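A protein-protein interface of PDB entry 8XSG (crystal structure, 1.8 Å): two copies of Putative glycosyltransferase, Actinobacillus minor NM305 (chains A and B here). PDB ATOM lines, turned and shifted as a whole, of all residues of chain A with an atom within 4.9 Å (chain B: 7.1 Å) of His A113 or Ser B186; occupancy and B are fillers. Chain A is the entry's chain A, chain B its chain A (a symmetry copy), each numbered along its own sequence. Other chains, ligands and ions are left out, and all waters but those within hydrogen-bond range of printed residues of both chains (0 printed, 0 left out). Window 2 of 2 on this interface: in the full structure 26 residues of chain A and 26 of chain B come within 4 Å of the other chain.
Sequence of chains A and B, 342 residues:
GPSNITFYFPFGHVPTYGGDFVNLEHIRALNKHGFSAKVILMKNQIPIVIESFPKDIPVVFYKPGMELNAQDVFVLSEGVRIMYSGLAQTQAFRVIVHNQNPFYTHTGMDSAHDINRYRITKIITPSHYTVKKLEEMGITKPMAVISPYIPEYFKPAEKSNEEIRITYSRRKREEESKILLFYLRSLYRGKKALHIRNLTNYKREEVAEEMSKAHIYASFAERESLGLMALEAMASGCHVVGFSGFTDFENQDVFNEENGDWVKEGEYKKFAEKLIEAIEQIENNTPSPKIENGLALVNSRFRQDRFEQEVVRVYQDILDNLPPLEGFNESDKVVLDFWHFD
No position is printed for both chains.
Printed residues of chain B within 4 Å of Ser A111: Phe B182 (3.6 Å) and Ser B186 (3.5 Å).
Of the printed residues of chain B, Ala A112 touches Phe B182 and Ser B186.
Of chain B, only Arg B185 (3.5 Å) and Ser B186 (3.0 Å) come within 4 Å of His A113.
Of the printed residues of chain A, Tyr B183 touches Met A137 (3.4 Å).
Of the printed residues of chain A, Ser B186 touches Ser A111 (3.5 Å), Ala A112 (2.8 Å), His A113 (3.0 Å) and Met A137 (3.4 Å).
The nearest residue of chain B that does not touch His A113 is Tyr B188 (4.6 Å).
The nearest printed residue of chain A that does not touch Arg B185 is Ser A111 (4.3 Å).
The side-chain hydroxyl of Ser B186 lies within hydrogen-bond range of the backbone NH of Ala A112, 2.8 Å away.
NE2 of His A113 lies within hydrogen-bond range of O of Ser B186.
OG of Ser A111 is in hydrogen-bond range of N of His A113 (3.0 Å).
The side-chain hydroxyl (OG) of Ser A111 is in hydrogen-bond range of the backbone NH (N) of Asp A114 (3.3 Å).
The side-chain amide nitrogen of Asn A116 sits close to the backbone carbonyl oxygen of Ala A112, 3.5 Å away.
The backbone carbonyl oxygen (O) of His A113 sits close to the guanidinium group (NE) of Arg A117 (3.4 Å).
The side-chain hydroxyl of Ser B186 sits at hydrogen-bond distance from the backbone carbonyl oxygen of Phe B182, at 2.8 Å.
CE2 of Phe B182 touches CA of Ser A111 (3.6 Å).
CA of Ser A111 touches OG of Ser B186, 3.5 Å away.
N of Ala A112 touches CZ of Phe B182, at 3.7 Å.
CE1 of His A113 touches O of Arg B185 (3.5 Å).
Met A137 touches Phe B182.
Tyr B183 touches Met A137 (CZ to CG, 3.4 Å).
Met A137 touches Ser B186.
Hydrophobic or aromatic side chains of chain B within 4 Å of the printed part of chain A: Phe B182 and Tyr B183.
Hydrophobic or aromatic side chains of chain A within 4 Å of the printed part of chain B: Ala A112, His A113 and Met A137.
Among the printed residues, no Asp or Glu carboxylate lies within 4 Å of a Lys or Arg side-chain nitrogen of the other chain.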
ATOM      1  N   SER A 111      -4.602  30.352  -7.432  1.00  0.00           N
ATOM      2  CA  SER A 111      -4.778  28.984  -6.988  1.00  0.00           C
ATOM      3  C   SER A 111      -5.260  28.944  -5.546  1.00  0.00           C
ATOM      4  O   SER A 111      -5.219  29.941  -4.840  1.00  0.00           O
ATOM      5  CB  SER A 111      -3.501  28.220  -7.121  1.00  0.00           C
ATOM      6  OG  SER A 111      -2.603  28.572  -6.089  1.00  0.00           O
ATOM      7  N   ALA A 112      -5.663  27.756  -5.107  1.00  0.00           N
ATOM      8  CA  ALA A 112      -5.934  27.545  -3.706  1.00  0.00           C
ATOM      9  C   ALA A 112      -4.712  27.909  -2.866  1.00  0.00           C
ATOM     10  O   ALA A 112      -4.878  28.415  -1.756  1.00  0.00           O
ATOM     11  CB  ALA A 112      -6.367  26.133  -3.471  1.00  0.00           C
ATOM     12  N   HIS A 113      -3.498  27.656  -3.385  1.00  0.00           N
ATOM     13  CA  HIS A 113      -2.290  27.838  -2.595  1.00  0.00           C
ATOM     14  C   HIS A 113      -2.099  29.312  -2.238  1.00  0.00           C
ATOM     15  O   HIS A 113      -1.664  29.621  -1.130  1.00  0.00           O
ATOM     16  CB  HIS A 113      -1.063  27.258  -3.315  1.00  0.00           C
ATOM     17  CG  HIS A 113      -1.260  25.851  -3.770  1.00  0.00           C
ATOM     18  ND1 HIS A 113      -1.098  25.433  -5.079  1.00  0.00           N
ATOM     19  CD2 HIS A 113      -1.650  24.775  -3.073  1.00  0.00           C
ATOM     20  CE1 HIS A 113      -1.357  24.141  -5.154  1.00  0.00           C
ATOM     21  NE2 HIS A 113      -1.700  23.721  -3.949  1.00  0.00           N
ATOM     22  N   ASP A 114      -2.447  30.209  -3.172  1.00  0.00           N
ATOM     23  CA  ASP A 114      -2.314  31.644  -2.979  1.00  0.00           C
ATOM     24  C   ASP A 114      -3.306  32.148  -1.934  1.00  0.00           C
ATOM     25  O   ASP A 114      -2.989  33.067  -1.197  1.00  0.00           O
ATOM     26  CB  ASP A 114      -2.523  32.408  -4.283  1.00  0.00           C
ATOM     27  CG  ASP A 114      -1.411  32.210  -5.288  1.00  0.00           C
ATOM     28  OD1 ASP A 114      -0.310  31.851  -4.885  1.00  0.00           O
ATOM     29  OD2 ASP A 114      -1.690  32.377  -6.460  1.00  0.00           O
ATOM     30  N   ILE A 115      -4.506  31.565  -1.910  1.00  0.00           N
ATOM     31  CA  ILE A 115      -5.508  31.878  -0.902  1.00  0.00           C
ATOM     32  C   ILE A 115      -5.049  31.405   0.472  1.00  0.00           C
ATOM     33  O   ILE A 115      -5.127  32.158   1.439  1.00  0.00           O
ATOM     34  CB  ILE A 115      -6.852  31.248  -1.316  1.00  0.00           C
ATOM     35  CG1 ILE A 115      -7.427  31.993  -2.519  1.00  0.00           C
ATOM     36  CG2 ILE A 115      -7.841  31.215  -0.147  1.00  0.00           C
ATOM     37  CD1 ILE A 115      -8.613  31.287  -3.153  1.00  0.00           C
ATOM     38  N   ASN A 116      -4.561  30.155   0.531  1.00  0.00           N
ATOM     39  CA  ASN A 116      -4.138  29.523   1.771  1.00  0.00           C
ATOM     40  C   ASN A 116      -2.960  30.296   2.379  1.00  0.00           C
ATOM     41  O   ASN A 116      -2.872  30.434   3.607  1.00  0.00           O
ATOM     42  CB  ASN A 116      -3.834  28.041   1.543  1.00  0.00           C
ATOM     43  CG  ASN A 116      -5.060  27.216   1.209  1.00  0.00           C
ATOM     44  OD1 ASN A 116      -6.183  27.648   1.453  1.00  0.00           O
ATOM     45  ND2 ASN A 116      -4.860  26.001   0.713  1.00  0.00           N
ATOM     46  N   ARG A 117      -2.103  30.893   1.538  1.00  0.00           N
ATOM     47  CA  ARG A 117      -0.924  31.588   2.044  1.00  0.00           C
ATOM     48  C   ARG A 117      -1.222  33.065   2.315  1.00  0.00           C
ATOM     49  O   ARG A 117      -0.443  33.705   2.993  1.00  0.00           O
ATOM     50  CB  ARG A 117       0.262  31.425   1.094  1.00  0.00           C
ATOM     51  CG  ARG A 117       0.821  30.002   1.081  1.00  0.00           C
ATOM     52  CD  ARG A 117       2.010  29.733   0.163  1.00  0.00           C
ATOM     53  NE  ARG A 117       1.686  29.075  -1.104  1.00  0.00           N
ATOM     54  CZ  ARG A 117       1.721  29.671  -2.290  1.00  0.00           C
ATOM     55  NH1 ARG A 117       1.859  30.986  -2.356  1.00  0.00           N
ATOM     56  NH2 ARG A 117       1.574  28.962  -3.397  1.00  0.00           N
ATOM     57  N   MET A 137     -11.839  22.637  -4.006  1.00  0.00           N
ATOM     58  CA  MET A 137     -10.788  23.295  -4.761  1.00  0.00           C
ATOM     59  C   MET A 137      -9.454  23.302  -4.017  1.00  0.00           C
ATOM     60  O   MET A 137      -8.446  23.689  -4.603  1.00  0.00           O
ATOM     61  CB  MET A 137     -11.172  24.747  -5.057  1.00  0.00           C
ATOM     62  CG  MET A 137     -12.263  24.870  -6.098  1.00  0.00           C
ATOM     63  SD  MET A 137     -12.874  26.559  -6.191  1.00  0.00           S
ATOM     64  CE  MET A 137     -14.371  26.317  -7.137  1.00  0.00           C
ATOM     65  N   LEU B 180     -11.595  25.086 -14.662  1.00  0.00           N
ATOM     66  CA  LEU B 180     -10.779  23.882 -14.720  1.00  0.00           C
ATOM     67  C   LEU B 180      -9.316  24.212 -14.446  1.00  0.00           C
ATOM     68  O   LEU B 180      -8.687  23.516 -13.655  1.00  0.00           O
ATOM     69  CB  LEU B 180     -10.999  23.185 -16.076  1.00  0.00           C
ATOM     70  CG  LEU B 180     -10.237  21.872 -16.328  1.00  0.00           C
ATOM     71  CD1 LEU B 180      -8.783  22.120 -16.715  1.00  0.00           C
ATOM     72  CD2 LEU B 180     -10.294  20.896 -15.167  1.00  0.00           C
ATOM     73  N   LEU B 181      -8.752  25.233 -15.098  1.00  0.00           N
ATOM     74  CA  LEU B 181      -7.329  25.476 -14.952  1.00  0.00           C
ATOM     75  C   LEU B 181      -7.030  25.888 -13.515  1.00  0.00           C
ATOM     76  O   LEU B 181      -5.958  25.575 -13.002  1.00  0.00           O
ATOM     77  CB  LEU B 181      -6.825  26.488 -15.998  1.00  0.00           C
ATOM     78  CG  LEU B 181      -6.791  25.942 -17.434  1.00  0.00           C
ATOM     79  CD1 LEU B 181      -6.481  27.026 -18.435  1.00  0.00           C
ATOM     80  CD2 LEU B 181      -5.799  24.804 -17.617  1.00  0.00           C
ATOM     81  N   PHE B 182      -7.997  26.549 -12.858  1.00  0.00           N
ATOM     82  CA  PHE B 182      -7.827  26.896 -11.458  1.00  0.00           C
ATOM     83  C   PHE B 182      -7.720  25.635 -10.610  1.00  0.00           C
ATOM     84  O   PHE B 182      -6.874  25.550  -9.730  1.00  0.00           O
ATOM     85  CB  PHE B 182      -8.974  27.809 -10.984  1.00  0.00           C
ATOM     86  CG  PHE B 182      -8.905  28.193  -9.529  1.00  0.00           C
ATOM     87  CD1 PHE B 182      -9.480  27.400  -8.562  1.00  0.00           C
ATOM     88  CD2 PHE B 182      -8.278  29.364  -9.125  1.00  0.00           C
ATOM     89  CE1 PHE B 182      -9.387  27.729  -7.223  1.00  0.00           C
ATOM     90  CE2 PHE B 182      -8.199  29.701  -7.784  1.00  0.00           C
ATOM     91  CZ  PHE B 182      -8.730  28.870  -6.836  1.00  0.00           C
ATOM     92  N   TYR B 183      -8.618  24.678 -10.832  1.00  0.00           N
ATOM     93  CA  TYR B 183      -8.556  23.411 -10.138  1.00  0.00           C
ATOM     94  C   TYR B 183      -7.231  22.699 -10.431  1.00  0.00           C
ATOM     95  O   TYR B 183      -6.606  22.173  -9.519  1.00  0.00           O
ATOM     96  CB  TYR B 183      -9.710  22.489 -10.506  1.00  0.00           C
ATOM     97  CG  TYR B 183     -11.032  22.633  -9.789  1.00  0.00           C
ATOM     98  CD1 TYR B 183     -11.942  23.628 -10.119  1.00  0.00           C
ATOM     99  CD2 TYR B 183     -11.400  21.746  -8.788  1.00  0.00           C
ATOM    100  CE1 TYR B 183     -13.191  23.695  -9.533  1.00  0.00           C
ATOM    101  CE2 TYR B 183     -12.638  21.819  -8.160  1.00  0.00           C
ATOM    102  CZ  TYR B 183     -13.529  22.803  -8.530  1.00  0.00           C
ATOM    103  OH  TYR B 183     -14.766  22.863  -7.961  1.00  0.00           O
ATOM    104  N   LEU B 184      -6.767  22.734 -11.686  1.00  0.00           N
ATOM    105  CA  LEU B 184      -5.546  22.025 -12.059  1.00  0.00           C
ATOM    106  C   LEU B 184      -4.338  22.644 -11.362  1.00  0.00           C
ATOM    107  O   LEU B 184      -3.531  21.911 -10.792  1.00  0.00           O
ATOM    108  CB  LEU B 184      -5.364  22.059 -13.581  1.00  0.00           C
ATOM    109  CG  LEU B 184      -4.132  21.326 -14.126  1.00  0.00           C
ATOM    110  CD1 LEU B 184      -4.167  19.841 -13.790  1.00  0.00           C
ATOM    111  CD2 LEU B 184      -4.031  21.509 -15.630  1.00  0.00           C
ATOM    112  N   ARG B 185      -4.239  23.989 -11.383  1.00  0.00           N
ATOM    113  CA  ARG B 185      -3.141  24.665 -10.704  1.00  0.00           C
ATOM    114  C   ARG B 185      -3.182  24.349  -9.208  1.00  0.00           C
ATOM    115  O   ARG B 185      -2.132  24.240  -8.585  1.00  0.00           O
ATOM    116  CB  ARG B 185      -3.175  26.186 -10.905  1.00  0.00           C
ATOM    117  CG  ARG B 185      -2.920  26.647 -12.330  1.00  0.00           C
ATOM    118  CD  ARG B 185      -2.771  28.148 -12.450  1.00  0.00           C
ATOM    119  NE  ARG B 185      -3.941  28.877 -11.986  1.00  0.00           N
ATOM    120  CZ  ARG B 185      -4.937  29.309 -12.758  1.00  0.00           C
ATOM    121  NH1 ARG B 185      -4.906  29.053 -14.046  1.00  0.00           N
ATOM    122  NH2 ARG B 185      -5.968  29.966 -12.233  1.00  0.00           N
ATOM    123  N   SER B 186      -4.395  24.212  -8.649  1.00  0.00           N
ATOM    124  CA  SER B 186      -4.607  24.045  -7.220  1.00  0.00           C
ATOM    125  C   SER B 186      -4.266  22.627  -6.771  1.00  0.00           C
ATOM    126  O   SER B 186      -3.823  22.436  -5.651  1.00  0.00           O
ATOM    127  CB  SER B 186      -6.029  24.424  -6.815  1.00  0.00           C
ATOM    128  OG  SER B 186      -6.277  25.814  -7.040  1.00  0.00           O
ATOM    129  N   LEU B 187      -4.488  21.625  -7.619  1.00  0.00           N
ATOM    130  CA  LEU B 187      -4.396  20.232  -7.177  1.00  0.00           C
ATOM    131  C   LEU B 187      -3.071  19.604  -7.603  1.00  0.00           C
ATOM    132  O   LEU B 187      -2.645  18.604  -7.031  1.00  0.00           O
ATOM    133  CB  LEU B 187      -5.621  19.473  -7.714  1.00  0.00           C
ATOM    134  CG  LEU B 187      -6.962  19.960  -7.140  1.00  0.00           C
ATOM    135  CD1 LEU B 187      -8.125  19.095  -7.602  1.00  0.00           C
ATOM    136  CD2 LEU B 187      -6.929  20.037  -5.601  1.00  0.00           C
ATOM    137  N   TYR B 188      -2.413  20.190  -8.605  1.00  0.00           N
ATOM    138  CA  TYR B 188      -1.221  19.588  -9.173  1.00  0.00           C
ATOM    139  C   TYR B 188      -0.029  19.916  -8.289  1.00  0.00           C
ATOM    140  O   TYR B 188       0.307  21.083  -8.108  1.00  0.00           O
ATOM    141  CB  TYR B 188      -1.002  20.077 -10.608  1.00  0.00           C
ATOM    142  CG  TYR B 188       0.299  19.638 -11.238  1.00  0.00           C
ATOM    143  CD1 TYR B 188       0.512  18.308 -11.607  1.00  0.00           C
ATOM    144  CD2 TYR B 188       1.336  20.562 -11.444  1.00  0.00           C
ATOM    145  CE1 TYR B 188       1.715  17.902 -12.175  1.00  0.00           C
ATOM    146  CE2 TYR B 188       2.536  20.177 -12.028  1.00  0.00           C
ATOM    147  CZ  TYR B 188       2.728  18.842 -12.392  1.00  0.00           C
ATOM    148  OH  TYR B 188       3.892  18.430 -12.994  1.00  0.00           O
ATOM    149  N   ARG B 189       0.610  18.876  -7.751  1.00  0.00           N
ATOM    150  CA  ARG B 189       1.762  19.090  -6.886  1.00  0.00           C
ATOM    151  C   ARG B 189       2.917  18.224  -7.387  1.00  0.00           C
ATOM    152  O   ARG B 189       3.719  17.756  -6.592  1.00  0.00           O
ATOM    153  CB  ARG B 189       1.374  18.903  -5.414  1.00  0.00           C
ATOM    154  CG  ARG B 189       0.784  17.550  -5.039  1.00  0.00           C
ATOM    155  CD  ARG B 189       0.145  17.627  -3.651  1.00  0.00           C
ATOM    156  NE  ARG B 189      -0.465  16.390  -3.161  1.00  0.00           N
ATOM    157  CZ  ARG B 189      -1.473  15.733  -3.739  1.00  0.00           C
ATOM    158  NH1 ARG B 189      -1.953  16.132  -4.902  1.00  0.00           N
ATOM    159  NH2 ARG B 189      -1.995  14.660  -3.162  1.00  0.00           N
ATOM    160  N   ILE B 276      -3.965  15.142 -14.319  1.00  0.00           N
ATOM    161  CA  ILE B 276      -2.760  14.818 -13.577  1.00  0.00           C
ATOM    162  C   ILE B 276      -2.386  13.348 -13.799  1.00  0.00           C
ATOM    163  O   ILE B 276      -1.226  13.038 -14.080  1.00  0.00           O
ATOM    164  CB  ILE B 276      -2.933  15.188 -12.091  1.00  0.00           C
ATOM    165  CG1 ILE B 276      -2.920  16.710 -11.919  1.00  0.00           C
ATOM    166  CG2 ILE B 276      -1.858  14.512 -11.261  1.00  0.00           C
ATOM    167  CD1 ILE B 276      -3.570  17.216 -10.650  1.00  0.00           C
